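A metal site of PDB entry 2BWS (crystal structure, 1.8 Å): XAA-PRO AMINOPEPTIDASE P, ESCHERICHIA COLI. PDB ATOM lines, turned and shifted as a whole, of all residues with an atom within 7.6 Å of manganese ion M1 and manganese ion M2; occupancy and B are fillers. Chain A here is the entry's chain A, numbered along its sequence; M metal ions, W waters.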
ATOM      1  N   TYR A 229      15.825   0.793  -2.830  1.00  0.00           N
ATOM      2  CA  TYR A 229      16.618  -0.171  -2.052  1.00  0.00           C
ATOM      3  C   TYR A 229      15.643  -1.229  -1.550  1.00  0.00           C
ATOM      4  O   TYR A 229      14.438  -1.030  -1.591  1.00  0.00           O
ATOM      5  CB  TYR A 229      17.319   0.471  -0.855  1.00  0.00           C
ATOM      6  CG  TYR A 229      16.410   1.265   0.032  1.00  0.00           C
ATOM      7  CD1 TYR A 229      16.090   2.585  -0.257  1.00  0.00           C
ATOM      8  CD2 TYR A 229      15.802   0.681   1.164  1.00  0.00           C
ATOM      9  CE1 TYR A 229      15.224   3.322   0.520  1.00  0.00           C
ATOM     10  CE2 TYR A 229      14.927   1.429   1.980  1.00  0.00           C
ATOM     11  CZ  TYR A 229      14.640   2.744   1.648  1.00  0.00           C
ATOM     12  OH  TYR A 229      13.793   3.508   2.419  1.00  0.00           O
ATOM     13  N   ILE A 232      12.550  -2.892   4.017  1.00  0.00           N
ATOM     14  CA  ILE A 232      12.759  -3.442   5.355  1.00  0.00           C
ATOM     15  C   ILE A 232      11.410  -3.345   6.080  1.00  0.00           C
ATOM     16  O   ILE A 232      10.851  -2.254   6.206  1.00  0.00           O
ATOM     17  CB  ILE A 232      13.809  -2.601   6.108  1.00  0.00           C
ATOM     18  CG1 ILE A 232      15.187  -2.756   5.457  1.00  0.00           C
ATOM     19  CG2 ILE A 232      13.815  -2.912   7.596  1.00  0.00           C
ATOM     20  CD1 ILE A 232      16.089  -1.567   5.608  1.00  0.00           C
ATOM     21  N   LEU A 242      19.158  -3.687  11.538  1.00  0.00           N
ATOM     22  CA  LEU A 242      19.067  -2.411  10.828  1.00  0.00           C
ATOM     23  C   LEU A 242      18.521  -2.486   9.387  1.00  0.00           C
ATOM     24  O   LEU A 242      17.651  -1.680   8.999  1.00  0.00           O
ATOM     25  CB  LEU A 242      20.440  -1.705  10.837  1.00  0.00           C
ATOM     26  CG  LEU A 242      20.876  -1.271  12.242  1.00  0.00           C
ATOM     27  CD1 LEU A 242      22.175  -0.488  12.163  1.00  0.00           C
ATOM     28  CD2 LEU A 242      19.792  -0.441  12.960  1.00  0.00           C
ATOM     29  N   ILE A 259       9.291   0.086   9.331  1.00  0.00           N
ATOM     30  CA  ILE A 259       9.302   0.007   7.883  1.00  0.00           C
ATOM     31  C   ILE A 259      10.250   1.071   7.331  1.00  0.00           C
ATOM     32  O   ILE A 259      10.039   2.267   7.570  1.00  0.00           O
ATOM     33  CB  ILE A 259       7.916   0.193   7.285  1.00  0.00           C
ATOM     34  CG1 ILE A 259       6.948  -0.858   7.841  1.00  0.00           C
ATOM     35  CG2 ILE A 259       7.980   0.115   5.769  1.00  0.00           C
ATOM     36  CD1 ILE A 259       5.571  -0.835   7.178  1.00  0.00           C
ATOM     37  N   ASP A 260      11.275   0.608   6.625  1.00  0.00           N
ATOM     38  CA  ASP A 260      12.220   1.483   5.931  1.00  0.00           C
ATOM     39  C   ASP A 260      12.070   1.140   4.453  1.00  0.00           C
ATOM     40  O   ASP A 260      12.401   0.038   4.027  1.00  0.00           O
ATOM     41  CB  ASP A 260      13.637   1.253   6.436  1.00  0.00           C
ATOM     42  CG  ASP A 260      14.626   2.348   5.978  1.00  0.00           C
ATOM     43  OD1 ASP A 260      14.351   3.096   5.011  1.00  0.00           O
ATOM     44  OD2 ASP A 260      15.694   2.465   6.626  1.00  0.00           O
ATOM     45  N   ALA A 261      11.452   2.049   3.699  1.00  0.00           N
ATOM     46  CA  ALA A 261      11.171   1.841   2.281  1.00  0.00           C
ATOM     47  C   ALA A 261      11.173   3.152   1.536  1.00  0.00           C
ATOM     48  O   ALA A 261      10.755   4.206   2.073  1.00  0.00           O
ATOM     49  CB  ALA A 261       9.818   1.147   2.079  1.00  0.00           C
ATOM     50  N   GLY A 262      11.607   3.089   0.279  1.00  0.00           N
ATOM     51  CA  GLY A 262      11.649   4.252  -0.585  1.00  0.00           C
ATOM     52  C   GLY A 262      11.521   3.884  -2.045  1.00  0.00           C
ATOM     53  O   GLY A 262      11.983   2.829  -2.485  1.00  0.00           O
ATOM     54  N   GLY A 270      13.536   8.163  -2.852  1.00  0.00           N
ATOM     55  CA  GLY A 270      12.919   8.464  -1.576  1.00  0.00           C
ATOM     56  C   GLY A 270      13.471   7.489  -0.547  1.00  0.00           C
ATOM     57  O   GLY A 270      14.035   6.433  -0.903  1.00  0.00           O
ATOM     58  N   ASP A 271      13.346   7.839   0.721  1.00  0.00           N
ATOM     59  CA  ASP A 271      13.881   7.019   1.802  1.00  0.00           C
ATOM     60  C   ASP A 271      13.180   7.417   3.102  1.00  0.00           C
ATOM     61  O   ASP A 271      13.577   8.374   3.766  1.00  0.00           O
ATOM     62  CB  ASP A 271      15.396   7.207   1.883  1.00  0.00           C
ATOM     63  CG  ASP A 271      16.052   6.384   2.980  1.00  0.00           C
ATOM     64  OD1 ASP A 271      15.407   5.574   3.679  1.00  0.00           O
ATOM     65  OD2 ASP A 271      17.283   6.553   3.142  1.00  0.00           O
ATOM     66  N   ILE A 272      12.141   6.679   3.469  1.00  0.00           N
ATOM     67  CA  ILE A 272      11.391   6.966   4.684  1.00  0.00           C
ATOM     68  C   ILE A 272      11.440   5.763   5.608  1.00  0.00           C
ATOM     69  O   ILE A 272      11.362   4.619   5.132  1.00  0.00           O
ATOM     70  CB  ILE A 272       9.907   7.317   4.364  1.00  0.00           C
ATOM     71  CG1 ILE A 272       9.784   8.661   3.632  1.00  0.00           C
ATOM     72  CG2 ILE A 272       9.048   7.307   5.640  1.00  0.00           C
ATOM     73  CD1 ILE A 272       8.376   9.010   3.241  1.00  0.00           C
ATOM     74  N   THR A 273      11.577   6.032   6.907  1.00  0.00           N
ATOM     75  CA  THR A 273      11.322   5.028   7.941  1.00  0.00           C
ATOM     76  C   THR A 273      10.208   5.523   8.850  1.00  0.00           C
ATOM     77  O   THR A 273      10.206   6.694   9.290  1.00  0.00           O
ATOM     78  CB  THR A 273      12.554   4.691   8.801  1.00  0.00           C
ATOM     79  OG1 THR A 273      13.688   4.414   7.964  1.00  0.00           O
ATOM     80  CG2 THR A 273      12.255   3.474   9.703  1.00  0.00           C
ATOM     81  N   GLY A 351      24.740   6.437  11.716  1.00  0.00           N
ATOM     82  CA  GLY A 351      24.734   7.879  11.486  1.00  0.00           C
ATOM     83  C   GLY A 351      23.328   8.462  11.476  1.00  0.00           C
ATOM     84  O   GLY A 351      22.341   7.761  11.187  1.00  0.00           O
ATOM     85  N   LEU A 352      23.235   9.745  11.801  1.00  0.00           N
ATOM     86  CA  LEU A 352      21.969  10.455  11.797  1.00  0.00           C
ATOM     87  C   LEU A 352      21.448  10.761  10.382  1.00  0.00           C
ATOM     88  O   LEU A 352      20.233  10.834  10.154  1.00  0.00           O
ATOM     89  CB  LEU A 352      22.120  11.782  12.562  1.00  0.00           C
ATOM     90  CG  LEU A 352      20.872  12.668  12.714  1.00  0.00           C
ATOM     91  CD1 LEU A 352      19.775  11.941  13.513  1.00  0.00           C
ATOM     92  CD2 LEU A 352      21.268  13.992  13.376  1.00  0.00           C
ATOM     93  N   SER A 353      22.377  10.972   9.456  1.00  0.00           N
ATOM     94  CA  SER A 353      22.052  11.534   8.155  1.00  0.00           C
ATOM     95  C   SER A 353      22.998  11.054   7.079  1.00  0.00           C
ATOM     96  O   SER A 353      24.204  11.023   7.293  1.00  0.00           O
ATOM     97  CB  SER A 353      22.132  13.065   8.221  1.00  0.00           C
ATOM     98  OG  SER A 353      21.127  13.603   9.046  1.00  0.00           O
ATOM     99  N   HIS A 354      22.439  10.719   5.926  1.00  0.00           N
ATOM    100  CA  HIS A 354      23.232  10.505   4.722  1.00  0.00           C
ATOM    101  C   HIS A 354      22.649  11.346   3.573  1.00  0.00           C
ATOM    102  O   HIS A 354      21.461  11.675   3.554  1.00  0.00           O
ATOM    103  CB  HIS A 354      23.310   9.013   4.347  1.00  0.00           C
ATOM    104  CG  HIS A 354      21.976   8.376   4.117  1.00  0.00           C
ATOM    105  ND1 HIS A 354      21.285   8.515   2.939  1.00  0.00           N
ATOM    106  CD2 HIS A 354      21.200   7.609   4.921  1.00  0.00           C
ATOM    107  CE1 HIS A 354      20.126   7.858   3.025  1.00  0.00           C
ATOM    108  NE2 HIS A 354      20.049   7.315   4.223  1.00  0.00           N
ATOM    109  N   TRP A 355      23.514  11.703   2.632  1.00  0.00           N
ATOM    110  CA  TRP A 355      23.092  12.353   1.393  1.00  0.00           C
ATOM    111  C   TRP A 355      22.078  11.463   0.663  1.00  0.00           C
ATOM    112  O   TRP A 355      22.104  10.223   0.787  1.00  0.00           O
ATOM    113  CB  TRP A 355      24.260  12.591   0.434  1.00  0.00           C
ATOM    114  CG  TRP A 355      25.500  13.268   0.989  1.00  0.00           C
ATOM    115  CD1 TRP A 355      26.778  12.825   0.851  1.00  0.00           C
ATOM    116  CD2 TRP A 355      25.570  14.510   1.721  1.00  0.00           C
ATOM    117  NE1 TRP A 355      27.655  13.702   1.466  1.00  0.00           N
ATOM    118  CE2 TRP A 355      26.949  14.751   1.998  1.00  0.00           C
ATOM    119  CE3 TRP A 355      24.628  15.443   2.154  1.00  0.00           C
ATOM    120  CZ2 TRP A 355      27.393  15.882   2.692  1.00  0.00           C
ATOM    121  CZ3 TRP A 355      25.078  16.573   2.860  1.00  0.00           C
ATOM    122  CH2 TRP A 355      26.448  16.784   3.115  1.00  0.00           C
ATOM    123  N   LEU A 356      21.214  12.115  -0.116  1.00  0.00           N
ATOM    124  CA  LEU A 356      20.156  11.417  -0.855  1.00  0.00           C
ATOM    125  C   LEU A 356      20.112  11.949  -2.288  1.00  0.00           C
ATOM    126  O   LEU A 356      20.221  13.165  -2.517  1.00  0.00           O
ATOM    127  CB  LEU A 356      18.822  11.664  -0.152  1.00  0.00           C
ATOM    128  CG  LEU A 356      17.583  10.935  -0.673  1.00  0.00           C
ATOM    129  CD1 LEU A 356      17.681   9.434  -0.403  1.00  0.00           C
ATOM    130  CD2 LEU A 356      16.324  11.516  -0.032  1.00  0.00           C
ATOM    131  N   VAL A 360      20.394   6.065  -2.889  1.00  0.00           N
ATOM    132  CA  VAL A 360      19.843   6.281  -1.569  1.00  0.00           C
ATOM    133  C   VAL A 360      20.938   6.731  -0.591  1.00  0.00           C
ATOM    134  O   VAL A 360      20.711   7.662   0.177  1.00  0.00           O
ATOM    135  CB  VAL A 360      19.016   5.061  -1.027  1.00  0.00           C
ATOM    136  CG1 VAL A 360      19.839   3.802  -0.941  1.00  0.00           C
ATOM    137  CG2 VAL A 360      18.389   5.403   0.308  1.00  0.00           C
ATOM    138  N   HIS A 361      22.092   6.064  -0.612  1.00  0.00           N
ATOM    139  CA  HIS A 361      23.264   6.568   0.085  1.00  0.00           C
ATOM    140  C   HIS A 361      24.077   7.354  -0.928  1.00  0.00           C
ATOM    141  O   HIS A 361      24.956   6.816  -1.624  1.00  0.00           O
ATOM    142  CB  HIS A 361      24.086   5.460   0.709  1.00  0.00           C
ATOM    143  CG  HIS A 361      23.370   4.705   1.772  1.00  0.00           C
ATOM    144  ND1 HIS A 361      23.702   3.422   2.116  1.00  0.00           N
ATOM    145  CD2 HIS A 361      22.300   5.043   2.542  1.00  0.00           C
ATOM    146  CE1 HIS A 361      22.892   3.003   3.076  1.00  0.00           C
ATOM    147  NE2 HIS A 361      22.026   3.966   3.353  1.00  0.00           N
ATOM    148  N   LEU A 380      19.450  15.389   2.173  1.00  0.00           N
ATOM    149  CA  LEU A 380      19.912  14.403   3.143  1.00  0.00           C
ATOM    150  C   LEU A 380      18.744  13.832   3.925  1.00  0.00           C
ATOM    151  O   LEU A 380      17.654  14.416   3.959  1.00  0.00           O
ATOM    152  CB  LEU A 380      20.953  14.986   4.101  1.00  0.00           C
ATOM    153  CG  LEU A 380      20.576  16.207   4.990  1.00  0.00           C
ATOM    154  CD1 LEU A 380      21.350  16.232   6.314  1.00  0.00           C
ATOM    155  CD2 LEU A 380      20.774  17.522   4.231  1.00  0.00           C
ATOM    156  N   THR A 381      18.988  12.682   4.531  1.00  0.00           N
ATOM    157  CA  THR A 381      18.021  12.071   5.428  1.00  0.00           C
ATOM    158  C   THR A 381      18.271  12.488   6.871  1.00  0.00           C
ATOM    159  O   THR A 381      19.341  12.979   7.203  1.00  0.00           O
ATOM    160  CB  THR A 381      18.073  10.535   5.350  1.00  0.00           C
ATOM    161  OG1 THR A 381      19.324  10.070   5.895  1.00  0.00           O
ATOM    162  CG2 THR A 381      17.911  10.071   3.904  1.00  0.00           C
ATOM    163  N   VAL A 382      17.275  12.290   7.714  1.00  0.00           N
ATOM    164  CA  VAL A 382      17.409  12.485   9.150  1.00  0.00           C
ATOM    165  C   VAL A 382      16.736  11.284   9.791  1.00  0.00           C
ATOM    166  O   VAL A 382      15.525  11.111   9.667  1.00  0.00           O
ATOM    167  CB  VAL A 382      16.724  13.806   9.617  1.00  0.00           C
ATOM    168  CG1 VAL A 382      17.026  14.111  11.059  1.00  0.00           C
ATOM    169  CG2 VAL A 382      17.137  14.981   8.699  1.00  0.00           C
ATOM    170  N   GLU A 383      17.537  10.405  10.391  1.00  0.00           N
ATOM    171  CA  GLU A 383      17.048   9.084  10.778  1.00  0.00           C
ATOM    172  C   GLU A 383      17.573   8.575  12.118  1.00  0.00           C
ATOM    173  O   GLU A 383      18.237   7.530  12.200  1.00  0.00           O
ATOM    174  CB  GLU A 383      17.324   8.070   9.663  1.00  0.00           C
ATOM    175  CG  GLU A 383      18.758   7.857   9.272  1.00  0.00           C
ATOM    176  CD  GLU A 383      18.828   6.936   8.059  1.00  0.00           C
ATOM    177  OE1 GLU A 383      18.366   5.780   8.156  1.00  0.00           O
ATOM    178  OE2 GLU A 383      19.252   7.410   7.000  1.00  0.00           O
ATOM    179  N   ARG A 404      13.032   3.426  14.484  1.00  0.00           N
ATOM    180  CA  ARG A 404      13.660   4.466  13.677  1.00  0.00           C
ATOM    181  C   ARG A 404      12.584   5.308  13.016  1.00  0.00           C
ATOM    182  O   ARG A 404      11.517   4.807  12.633  1.00  0.00           O
ATOM    183  CB  ARG A 404      14.615   3.841  12.652  1.00  0.00           C
ATOM    184  CG  ARG A 404      15.236   4.835  11.667  1.00  0.00           C
ATOM    185  CD  ARG A 404      16.440   4.268  10.904  1.00  0.00           C
ATOM    186  NE  ARG A 404      16.103   3.215   9.916  1.00  0.00           N
ATOM    187  CZ  ARG A 404      16.256   1.909  10.102  1.00  0.00           C
ATOM    188  NH1 ARG A 404      16.695   1.411  11.248  1.00  0.00           N
ATOM    189  NH2 ARG A 404      15.948   1.054   9.116  1.00  0.00           N
ATOM    190  N   GLU A 406      12.443   8.409  10.073  1.00  0.00           N
ATOM    191  CA  GLU A 406      13.324   9.008   9.066  1.00  0.00           C
ATOM    192  C   GLU A 406      12.544   9.842   8.066  1.00  0.00           C
ATOM    193  O   GLU A 406      11.585   9.347   7.445  1.00  0.00           O
ATOM    194  CB  GLU A 406      14.114   7.918   8.341  1.00  0.00           C
ATOM    195  CG  GLU A 406      14.814   8.375   7.074  1.00  0.00           C
ATOM    196  CD  GLU A 406      15.635   7.267   6.443  1.00  0.00           C
ATOM    197  OE1 GLU A 406      15.261   6.083   6.547  1.00  0.00           O
ATOM    198  OE2 GLU A 406      16.655   7.587   5.802  1.00  0.00           O
ATOM    199  N   ASP A 407      13.020  11.070   7.866  1.00  0.00           N
ATOM    200  CA  ASP A 407      12.510  11.996   6.842  1.00  0.00           C
ATOM    201  C   ASP A 407      13.650  12.372   5.890  1.00  0.00           C
ATOM    202  O   ASP A 407      14.817  12.233   6.231  1.00  0.00           O
ATOM    203  CB  ASP A 407      11.939  13.260   7.492  1.00  0.00           C
ATOM    204  CG  ASP A 407      10.516  13.091   8.014  1.00  0.00           C
ATOM    205  OD1 ASP A 407       9.748  12.231   7.505  1.00  0.00           O
ATOM    206  OD2 ASP A 407      10.157  13.829   8.946  1.00  0.00           O
ATOM    207  N   ASP A 408      13.274  12.869   4.712  1.00  0.00           N
ATOM    208  CA  ASP A 408      14.190  13.380   3.709  1.00  0.00           C
ATOM    209  C   ASP A 408      14.001  14.884   3.630  1.00  0.00           C
ATOM    210  O   ASP A 408      12.864  15.368   3.548  1.00  0.00           O
ATOM    211  CB  ASP A 408      13.919  12.752   2.339  1.00  0.00           C
ATOM    212  CG  ASP A 408      13.864  11.233   2.406  1.00  0.00           C
ATOM    213  OD1 ASP A 408      14.574  10.661   3.250  1.00  0.00           O
ATOM    214  OD2 ASP A 408      13.115  10.632   1.591  1.00  0.00           O
HETATM  215 MN    MN M   1      15.965   4.522   5.320  1.00  0.00          MN
HETATM  216 MN    MN M   2      18.265   6.554   5.116  1.00  0.00          MN
HETATM  217  O   HOH W   1      19.998   3.585   5.163  1.00  0.00           O
HETATM  218  O   HOH W   2      17.886   4.858   5.801  1.00  0.00           O
HETATM  219  O   HOH W   3      17.120   3.075   3.850  1.00  0.00           O
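Manganese ion M2 is bound by water W2 (1.9 Å), OE2 of Glu 406 (2.0 Å), NE2 of His 354 (2.1 Å), OD2 of Asp 271 (2.2 Å) and OE2 of Glu 383 (2.3 Å).
Merely in contact with manganese ion M2: Thr 381.
Within 4 Å of manganese ion M2: Asp 271, His 354, Thr 381, Glu 383 and Glu 406.
The nearest printed residue that does not touch manganese ion M2 is His 361 (4.9 Å).
Merely in contact with manganese ion M1: Thr 273 and Tyr 229.
Within 4 Å of manganese ion M1: Tyr 229, Asp 260, Asp 271, Thr 273, Glu 383 and Glu 406.
The backbone NH of Ala 261 sits close to the side-chain hydroxyl of Tyr 229, 3.0 Å away.
The side-chain carboxylate (OD1) of Asp 260 lies close to the side-chain hydroxyl (OH) of Tyr 229 (2.7 Å).
The backbone carbonyl oxygen of Thr 381 lies within hydrogen-bond range of the side-chain hydroxyl of Ser 353 (2.6 Å).
N of Gly 262 sits at hydrogen-bond distance from OH of Tyr 229, 3.1 Å away.
The backbone NH (N) of Glu 406 is in hydrogen-bond range of the backbone carbonyl oxygen (O) of Thr 273.
The backbone NH (N) of Thr 381 is in hydrogen-bond range of the backbone carbonyl oxygen (O) of His 354.
The side-chain hydroxyl (OG1) of Thr 273 sits at hydrogen-bond distance from the guanidinium group (NE) of Arg 404, 3.3 Å away.
N of Glu 383 sits at hydrogen-bond distance from O of Leu 352.
Manganese ion M1 is bound by water W2 (2.0 Å), OD1 of Asp 271 (2.0 Å), OE1 of Glu 406 (2.1 Å), OD1 of Asp 260 (2.2 Å), water W3 (2.4 Å) and OD2 of Asp 260 (2.5 Å).
Manganese ion M1 has six donor atoms within binding distance.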
